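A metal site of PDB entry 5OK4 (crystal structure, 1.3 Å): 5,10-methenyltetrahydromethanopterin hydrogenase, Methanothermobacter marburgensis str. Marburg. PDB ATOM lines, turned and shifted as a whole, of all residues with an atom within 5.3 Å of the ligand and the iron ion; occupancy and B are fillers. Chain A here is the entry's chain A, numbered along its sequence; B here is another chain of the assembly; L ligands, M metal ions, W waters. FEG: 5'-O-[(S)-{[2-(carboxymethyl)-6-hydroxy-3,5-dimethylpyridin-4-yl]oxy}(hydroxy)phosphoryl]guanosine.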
ATOM      1  N   LEU A   6      10.653 -15.964  -9.315  1.00  0.00           N
ATOM      2  CA  LEU A   6      10.265 -17.293  -8.837  1.00  0.00           C
ATOM      3  C   LEU A   6       8.829 -17.533  -9.282  1.00  0.00           C
ATOM      4  O   LEU A   6       7.866 -17.065  -8.654  1.00  0.00           O
ATOM      5  CB  LEU A   6      10.436 -17.402  -7.328  1.00  0.00           C
ATOM      6  CG  LEU A   6      11.808 -17.013  -6.780  1.00  0.00           C
ATOM      7  CD1 LEU A   6      11.875 -17.385  -5.298  1.00  0.00           C
ATOM      8  CD2 LEU A   6      12.938 -17.591  -7.505  1.00  0.00           C
ATOM      9  N   GLY A   7       8.708 -18.229 -10.407  1.00  0.00           N
ATOM     10  CA  GLY A   7       7.443 -18.531 -11.055  1.00  0.00           C
ATOM     11  C   GLY A   7       7.345 -17.842 -12.398  1.00  0.00           C
ATOM     12  O   GLY A   7       7.280 -16.612 -12.464  1.00  0.00           O
ATOM     13  N   ALA A   8       7.350 -18.639 -13.459  1.00  0.00           N
ATOM     14  CA  ALA A   8       7.265 -18.112 -14.821  1.00  0.00           C
ATOM     15  C   ALA A   8       5.849 -17.842 -15.270  1.00  0.00           C
ATOM     16  O   ALA A   8       5.647 -17.094 -16.246  1.00  0.00           O
ATOM     17  CB  ALA A   8       7.887 -19.130 -15.790  1.00  0.00           C
ATOM     18  N   GLY A   9       4.863 -18.456 -14.630  1.00  0.00           N
ATOM     19  CA  GLY A   9       3.476 -18.332 -15.025  1.00  0.00           C
ATOM     20  C   GLY A   9       3.077 -19.280 -16.143  1.00  0.00           C
ATOM     21  O   GLY A   9       3.897 -19.903 -16.808  1.00  0.00           O
ATOM     22  N   CYS A  10       1.770 -19.370 -16.341  1.00  0.00           N
ATOM     23  CA  CYS A  10       1.194 -20.083 -17.484  1.00  0.00           C
ATOM     24  C   CYS A  10       0.157 -19.182 -18.136  1.00  0.00           C
ATOM     25  O   CYS A  10      -0.599 -18.504 -17.447  1.00  0.00           O
ATOM     26  CB  CYS A  10       0.523 -21.382 -17.062  1.00  0.00           C
ATOM     27  SG  CYS A  10      -0.159 -22.314 -18.453  1.00  0.00           S
ATOM     28  N   THR A  13      -4.870 -19.458 -18.245  1.00  0.00           N
ATOM     29  CA  THR A  13      -6.032 -18.746 -17.695  1.00  0.00           C
ATOM     30  C   THR A  13      -6.190 -17.376 -18.339  1.00  0.00           C
ATOM     31  O   THR A  13      -7.296 -16.837 -18.378  1.00  0.00           O
ATOM     32  CB  THR A  13      -5.965 -18.586 -16.190  1.00  0.00           C
ATOM     33  OG1 THR A  13      -4.838 -17.782 -15.824  1.00  0.00           O
ATOM     34  CG2 THR A  13      -5.950 -19.921 -15.496  1.00  0.00           C
ATOM     35  N   HIS A  14      -5.091 -16.801 -18.837  1.00  0.00           N
ATOM     36  CA  HIS A  14      -5.225 -15.527 -19.560  1.00  0.00           C
ATOM     37  C   HIS A  14      -6.010 -15.751 -20.837  1.00  0.00           C
ATOM     38  O   HIS A  14      -6.992 -15.048 -21.121  1.00  0.00           O
ATOM     39  CB  HIS A  14      -3.845 -14.921 -19.852  1.00  0.00           C
ATOM     40  CG  HIS A  14      -3.026 -14.653 -18.622  1.00  0.00           C
ATOM     41  ND1 HIS A  14      -1.896 -13.853 -18.640  1.00  0.00           N
ATOM     42  CD2 HIS A  14      -3.168 -15.068 -17.340  1.00  0.00           C
ATOM     43  CE1 HIS A  14      -1.379 -13.801 -17.418  1.00  0.00           C
ATOM     44  NE2 HIS A  14      -2.138 -14.520 -16.612  1.00  0.00           N
ATOM     45  N   SER A  42       3.048 -12.470 -18.110  1.00  0.00           N
ATOM     46  CA  SER A  42       3.252 -12.673 -16.676  1.00  0.00           C
ATOM     47  C   SER A  42       4.599 -12.094 -16.238  1.00  0.00           C
ATOM     48  O   SER A  42       4.948 -10.963 -16.615  1.00  0.00           O
ATOM     49  CB  SER A  42       3.053 -14.111 -16.316  1.00  0.00           C
ATOM     50  OG  SER A  42       1.777 -14.568 -16.737  1.00  0.00           O
ATOM     51  N   ALA A  62      13.242 -19.032 -11.989  1.00  0.00           N
ATOM     52  CA  ALA A  62      13.177 -20.354 -11.371  1.00  0.00           C
ATOM     53  C   ALA A  62      11.729 -20.827 -11.386  1.00  0.00           C
ATOM     54  O   ALA A  62      10.820 -20.093 -10.998  1.00  0.00           O
ATOM     55  CB  ALA A  62      13.680 -20.327  -9.931  1.00  0.00           C
ATOM     56  N   ASP A  63      11.534 -22.052 -11.788  1.00  0.00           N
ATOM     57  CA  ASP A  63      10.205 -22.645 -11.759  1.00  0.00           C
ATOM     58  C   ASP A  63      10.402 -24.140 -11.923  1.00  0.00           C
ATOM     59  O   ASP A  63      11.199 -24.557 -12.778  1.00  0.00           O
ATOM     60  CB  ASP A  63       9.407 -22.092 -12.933  1.00  0.00           C
ATOM     61  CG  ASP A  63       7.933 -22.345 -12.828  1.00  0.00           C
ATOM     62  OD1 ASP A  63       7.528 -23.489 -12.584  1.00  0.00           O
ATOM     63  OD2 ASP A  63       7.162 -21.386 -12.995  1.00  0.00           O
ATOM     64  N   PRO A  64       9.717 -24.989 -11.160  1.00  0.00           N
ATOM     65  CA  PRO A  64       9.868 -26.437 -11.375  1.00  0.00           C
ATOM     66  C   PRO A  64       9.503 -26.859 -12.779  1.00  0.00           C
ATOM     67  O   PRO A  64       9.950 -27.917 -13.255  1.00  0.00           O
ATOM     68  CB  PRO A  64       8.931 -27.054 -10.332  1.00  0.00           C
ATOM     69  CG  PRO A  64       8.744 -26.011  -9.315  1.00  0.00           C
ATOM     70  CD  PRO A  64       8.795 -24.718 -10.044  1.00  0.00           C
ATOM     71  N   VAL A  65       8.689 -26.064 -13.484  1.00  0.00           N
ATOM     72  CA  VAL A  65       8.154 -26.503 -14.754  1.00  0.00           C
ATOM     73  C   VAL A  65       9.249 -26.671 -15.790  1.00  0.00           C
ATOM     74  O   VAL A  65       9.046 -27.384 -16.773  1.00  0.00           O
ATOM     75  CB  VAL A  65       7.066 -25.527 -15.243  1.00  0.00           C
ATOM     76  CG1 VAL A  65       7.658 -24.209 -15.748  1.00  0.00           C
ATOM     77  CG2 VAL A  65       6.226 -26.175 -16.298  1.00  0.00           C
ATOM     78  N   PRO A 110       0.391 -25.974 -14.197  1.00  0.00           N
ATOM     79  CA  PRO A 110       1.673 -25.734 -13.546  1.00  0.00           C
ATOM     80  C   PRO A 110       1.645 -26.272 -12.140  1.00  0.00           C
ATOM     81  O   PRO A 110       0.595 -26.222 -11.524  1.00  0.00           O
ATOM     82  CB  PRO A 110       1.809 -24.200 -13.550  1.00  0.00           C
ATOM     83  CG  PRO A 110       0.554 -23.689 -14.004  1.00  0.00           C
ATOM     84  CD  PRO A 110      -0.243 -24.738 -14.656  1.00  0.00           C
ATOM     85  N   PRO A 111       2.777 -26.756 -11.625  1.00  0.00           N
ATOM     86  CA  PRO A 111       4.122 -26.710 -12.191  1.00  0.00           C
ATOM     87  C   PRO A 111       4.497 -27.876 -13.094  1.00  0.00           C
ATOM     88  O   PRO A 111       5.665 -27.992 -13.426  1.00  0.00           O
ATOM     89  CB  PRO A 111       5.017 -26.689 -10.959  1.00  0.00           C
ATOM     90  CG  PRO A 111       4.277 -27.487  -9.986  1.00  0.00           C
ATOM     91  CD  PRO A 111       2.803 -27.195 -10.226  1.00  0.00           C
ATOM     92  N   ALA A 114       3.317 -25.613 -18.475  1.00  0.00           N
ATOM     93  CA  ALA A 114       3.083 -24.169 -18.569  1.00  0.00           C
ATOM     94  C   ALA A 114       3.198 -23.789 -20.025  1.00  0.00           C
ATOM     95  O   ALA A 114       3.998 -24.370 -20.766  1.00  0.00           O
ATOM     96  CB  ALA A 114       4.058 -23.352 -17.738  1.00  0.00           C
ATOM     97  N   ASP A 131      15.015 -22.919  -6.668  1.00  0.00           N
ATOM     98  CA  ASP A 131      14.768 -21.584  -6.113  1.00  0.00           C
ATOM     99  C   ASP A 131      15.941 -21.121  -5.249  1.00  0.00           C
ATOM    100  O   ASP A 131      16.217 -19.916  -5.172  1.00  0.00           O
ATOM    101  CB  ASP A 131      13.507 -21.599  -5.254  1.00  0.00           C
ATOM    102  CG  ASP A 131      12.241 -21.837  -6.050  1.00  0.00           C
ATOM    103  OD1 ASP A 131      12.247 -21.685  -7.273  1.00  0.00           O
ATOM    104  OD2 ASP A 131      11.209 -22.163  -5.424  1.00  0.00           O
ATOM    105  N   TRP A 144       5.927 -15.286  -7.605  1.00  0.00           N
ATOM    106  CA  TRP A 144       4.724 -15.351  -8.423  1.00  0.00           C
ATOM    107  C   TRP A 144       4.057 -16.704  -8.157  1.00  0.00           C
ATOM    108  O   TRP A 144       3.989 -17.572  -9.013  1.00  0.00           O
ATOM    109  CB  TRP A 144       5.076 -15.178  -9.896  1.00  0.00           C
ATOM    110  CG  TRP A 144       3.990 -14.835 -10.797  1.00  0.00           C
ATOM    111  CD1 TRP A 144       3.456 -15.628 -11.770  1.00  0.00           C
ATOM    112  CD2 TRP A 144       3.395 -13.552 -10.933  1.00  0.00           C
ATOM    113  NE1 TRP A 144       2.549 -14.909 -12.497  1.00  0.00           N
ATOM    114  CE2 TRP A 144       2.480 -13.638 -11.997  1.00  0.00           C
ATOM    115  CE3 TRP A 144       3.546 -12.343 -10.257  1.00  0.00           C
ATOM    116  CZ2 TRP A 144       1.721 -12.539 -12.404  1.00  0.00           C
ATOM    117  CZ3 TRP A 144       2.784 -11.277 -10.640  1.00  0.00           C
ATOM    118  CH2 TRP A 144       1.872 -11.377 -11.702  1.00  0.00           C
ATOM    119  N   PHE A 145       3.579 -16.861  -6.945  1.00  0.00           N
ATOM    120  CA  PHE A 145       3.167 -18.151  -6.465  1.00  0.00           C
ATOM    121  C   PHE A 145       1.642 -18.283  -6.401  1.00  0.00           C
ATOM    122  O   PHE A 145       0.937 -17.282  -6.270  1.00  0.00           O
ATOM    123  CB  PHE A 145       3.734 -18.400  -5.051  1.00  0.00           C
ATOM    124  CG  PHE A 145       5.247 -18.461  -4.977  1.00  0.00           C
ATOM    125  CD1 PHE A 145       6.016 -18.934  -6.037  1.00  0.00           C
ATOM    126  CD2 PHE A 145       5.892 -18.055  -3.831  1.00  0.00           C
ATOM    127  CE1 PHE A 145       7.394 -18.997  -5.930  1.00  0.00           C
ATOM    128  CE2 PHE A 145       7.260 -18.127  -3.722  1.00  0.00           C
ATOM    129  CZ  PHE A 145       8.018 -18.592  -4.764  1.00  0.00           C
ATOM    130  N   PRO A 146       1.202 -19.495  -6.566  1.00  0.00           N
ATOM    131  CA  PRO A 146      -0.127 -19.873  -6.169  1.00  0.00           C
ATOM    132  C   PRO A 146      -0.504 -19.413  -4.777  1.00  0.00           C
ATOM    133  O   PRO A 146       0.159 -18.694  -4.030  1.00  0.00           O
ATOM    134  CB  PRO A 146      -0.048 -21.408  -6.194  1.00  0.00           C
ATOM    135  CG  PRO A 146       0.974 -21.707  -7.214  1.00  0.00           C
ATOM    136  CD  PRO A 146       1.981 -20.656  -7.011  1.00  0.00           C
ATOM    137  N   ILE A 154       6.826 -23.312   0.188  1.00  0.00           N
ATOM    138  CA  ILE A 154       7.723 -22.986  -0.919  1.00  0.00           C
ATOM    139  C   ILE A 154       8.858 -22.109  -0.432  1.00  0.00           C
ATOM    140  O   ILE A 154      10.032 -22.353  -0.699  1.00  0.00           O
ATOM    141  CB  ILE A 154       6.920 -22.319  -2.062  1.00  0.00           C
ATOM    142  CG1 ILE A 154       5.912 -23.287  -2.694  1.00  0.00           C
ATOM    143  CG2 ILE A 154       7.869 -21.752  -3.120  1.00  0.00           C
ATOM    144  CD1 ILE A 154       4.889 -22.638  -3.608  1.00  0.00           C
ATOM    145  N   HIS A 170       5.503 -10.203  -3.438  1.00  0.00           N
ATOM    146  CA  HIS A 170       4.515 -11.276  -3.396  1.00  0.00           C
ATOM    147  C   HIS A 170       3.429 -11.090  -4.451  1.00  0.00           C
ATOM    148  O   HIS A 170       3.058  -9.976  -4.804  1.00  0.00           O
ATOM    149  CB  HIS A 170       3.847 -11.376  -2.032  1.00  0.00           C
ATOM    150  CG  HIS A 170       3.017 -10.197  -1.678  1.00  0.00           C
ATOM    151  ND1 HIS A 170       1.706 -10.070  -2.065  1.00  0.00           N
ATOM    152  CD2 HIS A 170       3.339  -9.076  -1.010  1.00  0.00           C
ATOM    153  CE1 HIS A 170       1.248  -8.905  -1.632  1.00  0.00           C
ATOM    154  NE2 HIS A 170       2.224  -8.282  -1.001  1.00  0.00           N
ATOM    155  N   ALA A 171       2.885 -12.216  -4.893  1.00  0.00           N
ATOM    156  CA  ALA A 171       1.729 -12.246  -5.775  1.00  0.00           C
ATOM    157  C   ALA A 171       0.452 -11.843  -5.024  1.00  0.00           C
ATOM    158  O   ALA A 171       0.370 -11.865  -3.799  1.00  0.00           O
ATOM    159  CB  ALA A 171       1.584 -13.656  -6.343  1.00  0.00           C
ATOM    160  N   CYS A 172      -0.577 -11.508  -5.783  1.00  0.00           N
ATOM    161  CA  CYS A 172      -1.839 -11.082  -5.185  1.00  0.00           C
ATOM    162  C   CYS A 172      -2.598 -12.227  -4.552  1.00  0.00           C
ATOM    163  O   CYS A 172      -3.657 -11.998  -3.958  1.00  0.00           O
ATOM    164  CB  CYS A 172      -2.720 -10.415  -6.224  1.00  0.00           C
ATOM    165  SG  CYS A 172      -3.349 -11.539  -7.514  1.00  0.00           S
ATOM    166  N   THR A 173      -2.109 -13.431  -4.686  1.00  0.00           N
ATOM    167  CA  THR A 173      -2.679 -14.628  -4.094  1.00  0.00           C
ATOM    168  C   THR A 173      -2.439 -14.686  -2.591  1.00  0.00           C
ATOM    169  O   THR A 173      -2.932 -15.615  -1.946  1.00  0.00           O
ATOM    170  CB  THR A 173      -2.034 -15.825  -4.755  1.00  0.00           C
ATOM    171  OG1 THR A 173      -0.622 -15.700  -4.622  1.00  0.00           O
ATOM    172  CG2 THR A 173      -2.429 -15.945  -6.237  1.00  0.00           C
ATOM    173  N   HIS A 203       3.050  -5.554  -8.331  1.00  0.00           N
ATOM    174  CA  HIS A 203       1.910  -6.287  -8.828  1.00  0.00           C
ATOM    175  C   HIS A 203       1.206  -5.508  -9.914  1.00  0.00           C
ATOM    176  O   HIS A 203       0.754  -4.387  -9.668  1.00  0.00           O
ATOM    177  CB  HIS A 203       0.948  -6.605  -7.715  1.00  0.00           C
ATOM    178  CG  HIS A 203      -0.207  -7.407  -8.209  1.00  0.00           C
ATOM    179  ND1 HIS A 203      -1.417  -6.849  -8.529  1.00  0.00           N
ATOM    180  CD2 HIS A 203      -0.315  -8.726  -8.497  1.00  0.00           C
ATOM    181  CE1 HIS A 203      -2.235  -7.789  -8.981  1.00  0.00           C
ATOM    182  NE2 HIS A 203      -1.587  -8.936  -8.983  1.00  0.00           N
ATOM    183  N   PRO A 204       1.048  -6.081 -11.088  1.00  0.00           N
ATOM    184  CA  PRO A 204       0.380  -5.375 -12.176  1.00  0.00           C
ATOM    185  C   PRO A 204      -1.117  -5.479 -12.026  1.00  0.00           C
ATOM    186  O   PRO A 204      -1.654  -6.491 -11.561  1.00  0.00           O
ATOM    187  CB  PRO A 204       0.831  -6.172 -13.400  1.00  0.00           C
ATOM    188  CG  PRO A 204       1.049  -7.571 -12.875  1.00  0.00           C
ATOM    189  CD  PRO A 204       1.542  -7.410 -11.495  1.00  0.00           C
ATOM    190  N   VAL A 207      -3.292  -8.221 -16.590  1.00  0.00           N
ATOM    191  CA  VAL A 207      -2.112  -9.041 -16.796  1.00  0.00           C
ATOM    192  C   VAL A 207      -1.053  -8.142 -17.410  1.00  0.00           C
ATOM    193  O   VAL A 207      -1.373  -7.237 -18.208  1.00  0.00           O
ATOM    194  CB  VAL A 207      -2.459 -10.277 -17.641  1.00  0.00           C
ATOM    195  CG1 VAL A 207      -3.452 -11.158 -16.873  1.00  0.00           C
ATOM    196  CG2 VAL A 207      -3.006  -9.906 -19.010  1.00  0.00           C
ATOM    197  N   ASP B 189      -7.329 -10.472 -10.920  1.00  0.00           N
ATOM    198  CA  ASP B 189      -6.914  -9.524 -11.920  1.00  0.00           C
ATOM    199  C   ASP B 189      -7.744  -9.594 -13.180  1.00  0.00           C
ATOM    200  O   ASP B 189      -7.620  -8.715 -14.028  1.00  0.00           O
ATOM    201  CB  ASP B 189      -5.455  -9.771 -12.284  1.00  0.00           C
ATOM    202  CG  ASP B 189      -4.561  -9.730 -11.061  1.00  0.00           C
ATOM    203  OD1 ASP B 189      -4.849  -8.909 -10.144  1.00  0.00           O
ATOM    204  OD2 ASP B 189      -3.594 -10.535 -10.981  1.00  0.00           O
HETATM  205  N1  FEG L   1      -1.126 -14.234 -11.837  1.00  0.00           N
HETATM  206  C2  FEG L   1      -1.639 -14.939 -12.835  1.00  0.00           C
HETATM  207  O2  FEG L   1      -2.245 -14.305 -13.822  1.00  0.00           O
HETATM  208  C3  FEG L   1      -1.565 -16.376 -12.843  1.00  0.00           C
HETATM  209  C3M FEG L   1      -2.185 -17.139 -13.959  1.00  0.00           C
HETATM  210  C4  FEG L   1      -0.837 -17.014 -11.774  1.00  0.00           C
HETATM  211  C5  FEG L   1      -0.306 -16.220 -10.707  1.00  0.00           C
HETATM  212  C5M FEG L   1       0.458 -16.911  -9.609  1.00  0.00           C
HETATM  213  C6  FEG L   1      -0.496 -14.780 -10.793  1.00  0.00           C
HETATM  214  C7  FEG L   1       0.081 -13.917  -9.720  1.00  0.00           C
HETATM  215  C8  FEG L   1      -0.515 -12.547  -9.547  1.00  0.00           C
HETATM  216  O28 FEG L   1      -1.408 -12.116 -10.310  1.00  0.00           O
HETATM  217  O18 FEG L   1      -0.099 -11.887  -8.560  1.00  0.00           O
HETATM  218  O3P FEG L   1      -0.701 -18.360 -11.753  1.00  0.00           O
HETATM  219  P1  FEG L   1       0.349 -19.129 -12.682  1.00  0.00           P
HETATM  220  O1P FEG L   1      -0.073 -20.569 -12.610  1.00  0.00           O
HETATM  221  O2P FEG L   1       0.423 -18.464 -14.004  1.00  0.00           O
HETATM  222  O5S FEG L   1       1.771 -18.928 -11.962  1.00  0.00           O
HETATM  223  C5S FEG L   1       2.194 -19.704 -10.833  1.00  0.00           C
HETATM  224  C4S FEG L   1       3.616 -20.162 -11.135  1.00  0.00           C
HETATM  225  C3S FEG L   1       3.671 -21.308 -12.154  1.00  0.00           C
HETATM  226  O3S FEG L   1       4.523 -21.028 -13.259  1.00  0.00           O
HETATM  227  C2S FEG L   1       4.178 -22.470 -11.292  1.00  0.00           C
HETATM  228  O2S FEG L   1       4.805 -23.535 -11.976  1.00  0.00           O
HETATM  229  C1S FEG L   1       5.059 -21.735 -10.300  1.00  0.00           C
HETATM  230  O4S FEG L   1       4.220 -20.652  -9.939  1.00  0.00           O
HETATM  231  N9A FEG L   1       5.422 -22.500  -9.108  1.00  0.00           N
HETATM  232  C8A FEG L   1       4.666 -23.417  -8.436  1.00  0.00           C
HETATM  233  N7A FEG L   1       5.390 -23.900  -7.409  1.00  0.00           N
HETATM  234  C5A FEG L   1       6.591 -23.290  -7.427  1.00  0.00           C
HETATM  235  C4A FEG L   1       6.586 -22.358  -8.532  1.00  0.00           C
HETATM  236  C6A FEG L   1       7.792 -23.338  -6.630  1.00  0.00           C
HETATM  237  O6A FEG L   1       7.932 -24.115  -5.653  1.00  0.00           O
HETATM  238  N1A FEG L   1       8.770 -22.492  -7.011  1.00  0.00           N
HETATM  239  C2A FEG L   1       8.693 -21.671  -8.069  1.00  0.00           C
HETATM  240  N3A FEG L   1       7.618 -21.580  -8.865  1.00  0.00           N
HETATM  241  N2A FEG L   1       9.756 -20.899  -8.345  1.00  0.00           N
HETATM  242 FE    FE M   1      -2.448 -10.682  -9.414  1.00  0.00          FE
HETATM  243  O   HOH W   1      -4.700 -13.347 -13.629  1.00  0.00           O
HETATM  244  O   HOH W   2       0.804 -15.814 -14.602  1.00  0.00           O
HETATM  245  O   HOH W   3       3.793 -25.781  -6.100  1.00  0.00           O
HETATM  246  O   HOH W   4       9.580 -25.606  -3.621  1.00  0.00           O
HETATM  247  O   HOH W   5      -2.802 -19.499 -16.222  1.00  0.00           O
HETATM  248  O   HOH W   6      -2.380 -21.090 -14.022  1.00  0.00           O
HETATM  249  O   HOH W   7      -0.750 -22.104 -10.536  1.00  0.00           O
HETATM  250  O   HOH W   8       6.797 -26.389  -5.042  1.00  0.00           O
HETATM  251  O   HOH W   9      10.733 -25.470  -6.453  1.00  0.00           O
HETATM  252  O   HOH W  10      -2.267 -19.422  -8.948  1.00  0.00           O
HETATM  253  O   HOH W  11      -0.486 -12.173 -14.894  1.00  0.00           O
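Water W2 lies within hydrogen-bond range of OG of Ser 42 (2.7 Å), O2P of the ligand (2.7 Å) and NE1 of Trp 144 (2.9 Å). Water W11 lies within hydrogen-bond range of O2 of the ligand and NE2 of His 14. Water W9 bridges O6A of the ligand (3.2 Å) and OD2 of Asp 131 (3.5 Å). Water W5 bridges the side-chain hydroxyl of Thr 13 (2.7 Å) and the backbone carbonyl oxygen of Cys 10 (2.7 Å).
An oxygen (O18) of the ligand lies within hydrogen-bond range of the backbone NH of Cys 172, 2.8 Å away. OD2 of Asp 63 lies within hydrogen-bond range of O3S of the ligand. NE2 of His 14 lies within hydrogen-bond range of O2 of the ligand, at 2.8 Å. The side-chain carboxylate (OD1) of Asp 131 is in hydrogen-bond range of a nitrogen (N2A) of the ligand, 2.8 Å away. O2P of the ligand sits at hydrogen-bond distance from N of Cys 10, at 2.8 Å. An oxygen (O3S) of the ligand sits at hydrogen-bond distance from the backbone NH (N) of Gly 9 (2.9 Å). O of Ala 62 lies within hydrogen-bond range of N2A of the ligand (3.0 Å).
N of Ala 8 lies within hydrogen-bond range of OD2 of Asp 63. The side-chain carboxylate (OD1) of Asp 63 is in hydrogen-bond range of the backbone NH (N) of Val 65, 3.0 Å away. O of Ala 62 is in hydrogen-bond range of N of Gly 7. N of Trp 144 lies within hydrogen-bond range of O of Leu 6 (2.8 Å). The side-chain hydroxyl (OG1) of Thr 173 lies within hydrogen-bond range of the backbone carbonyl oxygen (O) of Phe 145 (2.8 Å). O of Pro 146 is in hydrogen-bond range of OG1 of Thr 173.
O of Trp 144 sits close to O4S of the ligand (3.2 Å). Residues that only touch the ligand: Leu 6 (3.6 Å), Gly 7 (3.5 Å), Ala 8 (3.7 Å), Thr 13 (3.3 Å), Pro 64 (3.6 Å), Pro 110 (3.4 Å), Pro 111 (3.3 Å), Phe 145 (3.4 Å), Pro 146 (3.7 Å), Ile 154 (3.5 Å) and Ala 171 (3.3 Å). Hydrophobic or aromatic side chains within 4 Å of the ligand: Leu 6, His 14, Pro 64, Pro 110, Pro 111, Trp 144, Phe 145, Pro 146, Ile 154, Ala 171 and His 203. 21 residues have an atom within 4 Å of the ligand: Leu 6, Gly 7, Ala 8, Gly 9, Cys 10, Thr 13, His 14, Ala 62, Asp 63, Pro 64, Pro 110, Pro 111, Asp 131, Trp 144, Phe 145, Pro 146, Ile 154, Ala 171, Cys 172, His 203 and Asp 189 of chain B.
The iron ion is bound by OD2 of Asp 189 of chain B (1.9 Å). The iron ion is bound by O28 of the ligand, at 2.0 Å. NE2 of His 203 is bound to the iron ion, 2.0 Å away. SG of Cys 172 binds the iron ion (2.3 Å). The iron ion has four donor atoms within binding distance. Slightly farther from the iron ion lies an oxygen (O18) of the ligand (2.8 Å).
Within 4 Å of the iron ion: Cys 172, His 203 and Asp 189 of chain B. Along chain A the residues within 4 Å of the iron ion span positions 172 to 203. The nearest printed residue that does not touch the iron ion is Pro 204 (4.8 Å).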
